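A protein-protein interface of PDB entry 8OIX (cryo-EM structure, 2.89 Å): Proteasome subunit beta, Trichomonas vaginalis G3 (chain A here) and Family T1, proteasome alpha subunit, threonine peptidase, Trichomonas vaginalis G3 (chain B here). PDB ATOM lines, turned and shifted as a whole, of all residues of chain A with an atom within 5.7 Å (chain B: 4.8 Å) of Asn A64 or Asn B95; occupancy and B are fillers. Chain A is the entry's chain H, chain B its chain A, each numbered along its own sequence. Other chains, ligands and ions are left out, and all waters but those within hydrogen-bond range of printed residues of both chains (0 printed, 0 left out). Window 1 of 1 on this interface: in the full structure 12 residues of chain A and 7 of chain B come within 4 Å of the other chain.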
ATOM      1  N   GLN A  38      12.566 -22.088  30.391  1.00  0.00           N
ATOM      2  CA  GLN A  38      11.849 -23.072  29.594  1.00  0.00           C
ATOM      3  C   GLN A  38      10.468 -23.239  30.219  1.00  0.00           C
ATOM      4  O   GLN A  38      10.266 -22.816  31.365  1.00  0.00           O
ATOM      5  CB  GLN A  38      12.612 -24.399  29.550  1.00  0.00           C
ATOM      6  CG  GLN A  38      14.050 -24.286  29.086  1.00  0.00           C
ATOM      7  CD  GLN A  38      14.445 -25.406  28.148  1.00  0.00           C
ATOM      8  OE1 GLN A  38      14.139 -26.572  28.391  1.00  0.00           O
ATOM      9  NE2 GLN A  38      15.125 -25.055  27.064  1.00  0.00           N
ATOM     10  N   VAL A  59      21.222 -18.405  29.533  1.00  0.00           N
ATOM     11  CA  VAL A  59      20.884 -19.782  29.868  1.00  0.00           C
ATOM     12  C   VAL A  59      19.791 -20.308  28.956  1.00  0.00           C
ATOM     13  O   VAL A  59      19.782 -21.494  28.620  1.00  0.00           O
ATOM     14  CB  VAL A  59      20.503 -19.883  31.352  1.00  0.00           C
ATOM     15  CG1 VAL A  59      19.981 -21.266  31.684  1.00  0.00           C
ATOM     16  CG2 VAL A  59      21.723 -19.601  32.168  1.00  0.00           C
ATOM     17  N   LYS A  60      18.862 -19.452  28.531  1.00  0.00           N
ATOM     18  CA  LYS A  60      17.939 -19.871  27.482  1.00  0.00           C
ATOM     19  C   LYS A  60      18.705 -20.257  26.223  1.00  0.00           C
ATOM     20  O   LYS A  60      18.433 -21.298  25.612  1.00  0.00           O
ATOM     21  CB  LYS A  60      16.937 -18.758  27.180  1.00  0.00           C
ATOM     22  CG  LYS A  60      15.823 -18.630  28.197  1.00  0.00           C
ATOM     23  CD  LYS A  60      14.892 -17.481  27.857  1.00  0.00           C
ATOM     24  CE  LYS A  60      14.314 -17.632  26.460  1.00  0.00           C
ATOM     25  NZ  LYS A  60      13.759 -18.995  26.235  1.00  0.00           N
ATOM     26  N   ASN A  61      19.690 -19.441  25.844  1.00  0.00           N
ATOM     27  CA  ASN A  61      20.522 -19.760  24.688  1.00  0.00           C
ATOM     28  C   ASN A  61      21.292 -21.061  24.894  1.00  0.00           C
ATOM     29  O   ASN A  61      21.383 -21.885  23.982  1.00  0.00           O
ATOM     30  CB  ASN A  61      21.486 -18.609  24.407  1.00  0.00           C
ATOM     31  CG  ASN A  61      22.282 -18.813  23.135  1.00  0.00           C
ATOM     32  OD1 ASN A  61      21.877 -19.563  22.248  1.00  0.00           O
ATOM     33  ND2 ASN A  61      23.424 -18.145  23.041  1.00  0.00           N
ATOM     34  N   TYR A  62      21.848 -21.261  26.090  1.00  0.00           N
ATOM     35  CA  TYR A  62      22.650 -22.450  26.367  1.00  0.00           C
ATOM     36  C   TYR A  62      21.794 -23.710  26.394  1.00  0.00           C
ATOM     37  O   TYR A  62      22.245 -24.776  25.968  1.00  0.00           O
ATOM     38  CB  TYR A  62      23.392 -22.284  27.692  1.00  0.00           C
ATOM     39  CG  TYR A  62      24.797 -21.740  27.565  1.00  0.00           C
ATOM     40  CD1 TYR A  62      25.023 -20.411  27.235  1.00  0.00           C
ATOM     41  CD2 TYR A  62      25.900 -22.554  27.787  1.00  0.00           C
ATOM     42  CE1 TYR A  62      26.306 -19.909  27.123  1.00  0.00           C
ATOM     43  CE2 TYR A  62      27.186 -22.062  27.681  1.00  0.00           C
ATOM     44  CZ  TYR A  62      27.384 -20.740  27.347  1.00  0.00           C
ATOM     45  OH  TYR A  62      28.665 -20.247  27.238  1.00  0.00           O
ATOM     46  N   LEU A  63      20.566 -23.613  26.900  1.00  0.00           N
ATOM     47  CA  LEU A  63      19.684 -24.773  26.930  1.00  0.00           C
ATOM     48  C   LEU A  63      19.118 -25.084  25.556  1.00  0.00           C
ATOM     49  O   LEU A  63      18.876 -26.255  25.243  1.00  0.00           O
ATOM     50  CB  LEU A  63      18.546 -24.555  27.928  1.00  0.00           C
ATOM     51  CG  LEU A  63      18.933 -24.542  29.404  1.00  0.00           C
ATOM     52  CD1 LEU A  63      17.704 -24.381  30.271  1.00  0.00           C
ATOM     53  CD2 LEU A  63      19.669 -25.813  29.765  1.00  0.00           C
ATOM     54  N   ASN A  64      18.890 -24.063  24.728  1.00  0.00           N
ATOM     55  CA  ASN A  64      18.558 -24.326  23.334  1.00  0.00           C
ATOM     56  C   ASN A  64      19.742 -24.942  22.599  1.00  0.00           C
ATOM     57  O   ASN A  64      19.562 -25.808  21.735  1.00  0.00           O
ATOM     58  CB  ASN A  64      18.097 -23.040  22.653  1.00  0.00           C
ATOM     59  CG  ASN A  64      16.865 -22.445  23.298  1.00  0.00           C
ATOM     60  OD1 ASN A  64      16.093 -23.144  23.953  1.00  0.00           O
ATOM     61  ND2 ASN A  64      16.668 -21.146  23.107  1.00  0.00           N
ATOM     62  N   ALA A  65      20.960 -24.502  22.925  1.00  0.00           N
ATOM     63  CA  ALA A  65      22.159 -25.112  22.360  1.00  0.00           C
ATOM     64  C   ALA A  65      22.277 -26.569  22.780  1.00  0.00           C
ATOM     65  O   ALA A  65      22.696 -27.423  21.989  1.00  0.00           O
ATOM     66  CB  ALA A  65      23.399 -24.327  22.786  1.00  0.00           C
ATOM     67  N   LEU A  66      21.931 -26.866  24.033  1.00  0.00           N
ATOM     68  CA  LEU A  66      21.882 -28.244  24.502  1.00  0.00           C
ATOM     69  C   LEU A  66      20.945 -29.085  23.649  1.00  0.00           C
ATOM     70  O   LEU A  66      21.149 -30.295  23.505  1.00  0.00           O
ATOM     71  CB  LEU A  66      21.439 -28.267  25.965  1.00  0.00           C
ATOM     72  CG  LEU A  66      21.240 -29.606  26.667  1.00  0.00           C
ATOM     73  CD1 LEU A  66      22.556 -30.326  26.827  1.00  0.00           C
ATOM     74  CD2 LEU A  66      20.578 -29.394  28.015  1.00  0.00           C
ATOM     75  N   ASN A  67      19.926 -28.460  23.068  1.00  0.00           N
ATOM     76  CA  ASN A  67      18.925 -29.143  22.265  1.00  0.00           C
ATOM     77  C   ASN A  67      19.261 -29.168  20.780  1.00  0.00           C
ATOM     78  O   ASN A  67      18.510 -29.764  20.004  1.00  0.00           O
ATOM     79  CB  ASN A  67      17.559 -28.485  22.475  1.00  0.00           C
ATOM     80  CG  ASN A  67      17.143 -28.465  23.930  1.00  0.00           C
ATOM     81  OD1 ASN A  67      17.508 -29.350  24.703  1.00  0.00           O
ATOM     82  ND2 ASN A  67      16.376 -27.453  24.312  1.00  0.00           N
ATOM     83  N   ILE A  68      20.359 -28.529  20.366  1.00  0.00           N
ATOM     84  CA  ILE A  68      20.736 -28.538  18.953  1.00  0.00           C
ATOM     85  C   ILE A  68      20.993 -29.960  18.476  1.00  0.00           C
ATOM     86  O   ILE A  68      20.606 -30.338  17.363  1.00  0.00           O
ATOM     87  CB  ILE A  68      21.963 -27.642  18.710  1.00  0.00           C
ATOM     88  CG1 ILE A  68      21.629 -26.176  18.947  1.00  0.00           C
ATOM     89  CG2 ILE A  68      22.481 -27.815  17.305  1.00  0.00           C
ATOM     90  CD1 ILE A  68      22.837 -25.267  18.877  1.00  0.00           C
ATOM     91  N   ARG B  91      18.545 -25.313  14.169  1.00  0.00           N
ATOM     92  CA  ARG B  91      18.464 -25.096  15.605  1.00  0.00           C
ATOM     93  C   ARG B  91      19.440 -24.013  16.047  1.00  0.00           C
ATOM     94  O   ARG B  91      19.107 -23.197  16.911  1.00  0.00           O
ATOM     95  CB  ARG B  91      18.704 -26.409  16.345  1.00  0.00           C
ATOM     96  CG  ARG B  91      17.562 -27.394  16.166  1.00  0.00           C
ATOM     97  CD  ARG B  91      17.915 -28.773  16.673  1.00  0.00           C
ATOM     98  NE  ARG B  91      16.812 -29.708  16.494  1.00  0.00           N
ATOM     99  CZ  ARG B  91      16.892 -31.013  16.712  1.00  0.00           C
ATOM    100  NH1 ARG B  91      18.020 -31.579  17.109  1.00  0.00           N
ATOM    101  NH2 ARG B  91      15.815 -31.769  16.527  1.00  0.00           N
ATOM    102  N   SER B  92      20.641 -23.965  15.459  1.00  0.00           N
ATOM    103  CA  SER B  92      21.563 -22.879  15.776  1.00  0.00           C
ATOM    104  C   SER B  92      21.001 -21.530  15.340  1.00  0.00           C
ATOM    105  O   SER B  92      21.112 -20.540  16.072  1.00  0.00           O
ATOM    106  CB  SER B  92      22.918 -23.132  15.119  1.00  0.00           C
ATOM    107  OG  SER B  92      22.868 -22.852  13.733  1.00  0.00           O
ATOM    108  N   PHE B  93      20.399 -21.472  14.149  1.00  0.00           N
ATOM    109  CA  PHE B  93      19.732 -20.254  13.700  1.00  0.00           C
ATOM    110  C   PHE B  93      18.661 -19.829  14.691  1.00  0.00           C
ATOM    111  O   PHE B  93      18.574 -18.656  15.068  1.00  0.00           O
ATOM    112  CB  PHE B  93      19.104 -20.469  12.323  1.00  0.00           C
ATOM    113  CG  PHE B  93      20.090 -20.535  11.198  1.00  0.00           C
ATOM    114  CD1 PHE B  93      21.373 -20.041  11.346  1.00  0.00           C
ATOM    115  CD2 PHE B  93      19.724 -21.078   9.979  1.00  0.00           C
ATOM    116  CE1 PHE B  93      22.272 -20.097  10.302  1.00  0.00           C
ATOM    117  CE2 PHE B  93      20.617 -21.136   8.934  1.00  0.00           C
ATOM    118  CZ  PHE B  93      21.890 -20.642   9.093  1.00  0.00           C
ATOM    119  N   ALA B  94      17.830 -20.780  15.115  1.00  0.00           N
ATOM    120  CA  ALA B  94      16.734 -20.477  16.024  1.00  0.00           C
ATOM    121  C   ALA B  94      17.247 -19.983  17.368  1.00  0.00           C
ATOM    122  O   ALA B  94      16.703 -19.029  17.934  1.00  0.00           O
ATOM    123  CB  ALA B  94      15.870 -21.720  16.206  1.00  0.00           C
ATOM    124  N   ASN B  95      18.295 -20.617  17.896  1.00  0.00           N
ATOM    125  CA  ASN B  95      18.833 -20.201  19.186  1.00  0.00           C
ATOM    126  C   ASN B  95      19.486 -18.832  19.101  1.00  0.00           C
ATOM    127  O   ASN B  95      19.313 -18.004  19.999  1.00  0.00           O
ATOM    128  CB  ASN B  95      19.830 -21.231  19.702  1.00  0.00           C
ATOM    129  CG  ASN B  95      19.283 -22.628  19.667  1.00  0.00           C
ATOM    130  OD1 ASN B  95      18.087 -22.834  19.460  1.00  0.00           O
ATOM    131  ND2 ASN B  95      20.148 -23.602  19.873  1.00  0.00           N
ATOM    132  N   ASN B  96      20.252 -18.580  18.038  1.00  0.00           N
ATOM    133  CA  ASN B  96      20.857 -17.264  17.872  1.00  0.00           C
ATOM    134  C   ASN B  96      19.788 -16.191  17.714  1.00  0.00           C
ATOM    135  O   ASN B  96      19.900 -15.100  18.286  1.00  0.00           O
ATOM    136  CB  ASN B  96      21.805 -17.282  16.673  1.00  0.00           C
ATOM    137  CG  ASN B  96      22.613 -16.009  16.547  1.00  0.00           C
ATOM    138  OD1 ASN B  96      22.444 -15.243  15.600  1.00  0.00           O
ATOM    139  ND2 ASN B  96      23.501 -15.775  17.507  1.00  0.00           N
ATOM    140  N   PHE B  97      18.729 -16.495  16.962  1.00  0.00           N
ATOM    141  CA  PHE B  97      17.640 -15.542  16.791  1.00  0.00           C
ATOM    142  C   PHE B  97      16.925 -15.279  18.109  1.00  0.00           C
ATOM    143  O   PHE B  97      16.574 -14.137  18.411  1.00  0.00           O
ATOM    144  CB  PHE B  97      16.661 -16.051  15.733  1.00  0.00           C
ATOM    145  CG  PHE B  97      15.566 -15.081  15.403  1.00  0.00           C
ATOM    146  CD1 PHE B  97      14.422 -15.010  16.176  1.00  0.00           C
ATOM    147  CD2 PHE B  97      15.687 -14.230  14.322  1.00  0.00           C
ATOM    148  CE1 PHE B  97      13.422 -14.119  15.874  1.00  0.00           C
ATOM    149  CE2 PHE B  97      14.688 -13.334  14.017  1.00  0.00           C
ATOM    150  CZ  PHE B  97      13.554 -13.280  14.794  1.00  0.00           C
ATOM    151  N   GLU B  98      16.674 -16.325  18.896  1.00  0.00           N
ATOM    152  CA  GLU B  98      16.003 -16.126  20.174  1.00  0.00           C
ATOM    153  C   GLU B  98      16.897 -15.391  21.163  1.00  0.00           C
ATOM    154  O   GLU B  98      16.401 -14.638  22.006  1.00  0.00           O
ATOM    155  CB  GLU B  98      15.550 -17.470  20.745  1.00  0.00           C
ATOM    156  CG  GLU B  98      14.989 -17.393  22.156  1.00  0.00           C
ATOM    157  CD  GLU B  98      14.056 -18.541  22.478  1.00  0.00           C
ATOM    158  OE1 GLU B  98      12.875 -18.480  22.078  1.00  0.00           O
ATOM    159  OE2 GLU B  98      14.504 -19.506  23.132  1.00  0.00           O
ATOM    160  N   TYR B  99      18.212 -15.593  21.080  1.00  0.00           N
ATOM    161  CA  TYR B  99      19.120 -14.883  21.972  1.00  0.00           C
ATOM    162  C   TYR B  99      19.215 -13.408  21.603  1.00  0.00           C
ATOM    163  O   TYR B  99      19.320 -12.549  22.486  1.00  0.00           O
ATOM    164  CB  TYR B  99      20.500 -15.537  21.946  1.00  0.00           C
ATOM    165  CG  TYR B  99      21.512 -14.854  22.833  1.00  0.00           C
ATOM    166  CD1 TYR B  99      21.472 -15.012  24.210  1.00  0.00           C
ATOM    167  CD2 TYR B  99      22.509 -14.054  22.295  1.00  0.00           C
ATOM    168  CE1 TYR B  99      22.393 -14.391  25.027  1.00  0.00           C
ATOM    169  CE2 TYR B  99      23.435 -13.429  23.104  1.00  0.00           C
ATOM    170  CZ  TYR B  99      23.373 -13.601  24.469  1.00  0.00           C
ATOM    171  OH  TYR B  99      24.295 -12.980  25.278  1.00  0.00           O
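O of Asn A67 is in hydrogen-bond range of NH1 of Arg B91.
The backbone carbonyl oxygen (O) of Ile A68 is in hydrogen-bond range of the guanidinium group (NH1) of Arg B91 (2.9 Å).
The side-chain amide nitrogen (ND2) of Asn B95 sits at hydrogen-bond distance from the backbone carbonyl oxygen (O) of Asn A64, 2.9 Å away.
The side-chain amide nitrogen (ND2) of Asn B95 sits close to the backbone NH (N) of Ala A65.
The side-chain amino group of Lys A60 lies within salt-bridge range of the side-chain carboxylate of Glu B98 (3.2 Å).
ND2 of Asn A64 lies within hydrogen-bond range of OE2 of Glu B98, at 2.7 Å.
Asn A64 touches just these residues of chain B: Asn B95 and Glu B98.
Of chain A, only Asn A61, Asn A64, Ala A65 and Ile A68 come within 4 Å of Asn B95.
Printed residues of chain B within 4 Å of Lys A60: Glu B98.
Of the printed residues of chain B, Asn A67 touches Arg B91 (3.5 Å).
Of the printed residues of chain A, Glu B98 touches Lys A60 (3.2 Å) and Asn A64 (2.7 Å).
Phe B97 touches none of the printed residues of chain A.
The backbone carbonyl oxygen (O) of Arg B91 lies close to the side-chain amide oxygen (OD1) of Asn B95 (2.8 Å).
ND2 of Asn A64 sits close to O of Lys A60 (3.1 Å).
O of Leu A63 lies within hydrogen-bond range of ND2 of Asn A67 (2.9 Å).
Of the 11 printed residues of chain A, 6 touch a printed residue of chain B.
Of the 9 printed residues of chain B, 4 touch a printed residue of chain A.
Among the printed residues, 9 pairs touch across the chains.
Among the printed residues, Asp or Glu carboxylates within 4 Å of a Lys or Arg side-chain nitrogen of the other chain: Lys A60 with Glu B98.
Asn A61 touches Asn B95 (OD1 to CB, 3.7 Å).
Asn A61 touches Tyr B99.
Ile A68 touches Asn B95 (CG1 to ND2, 3.1 Å).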
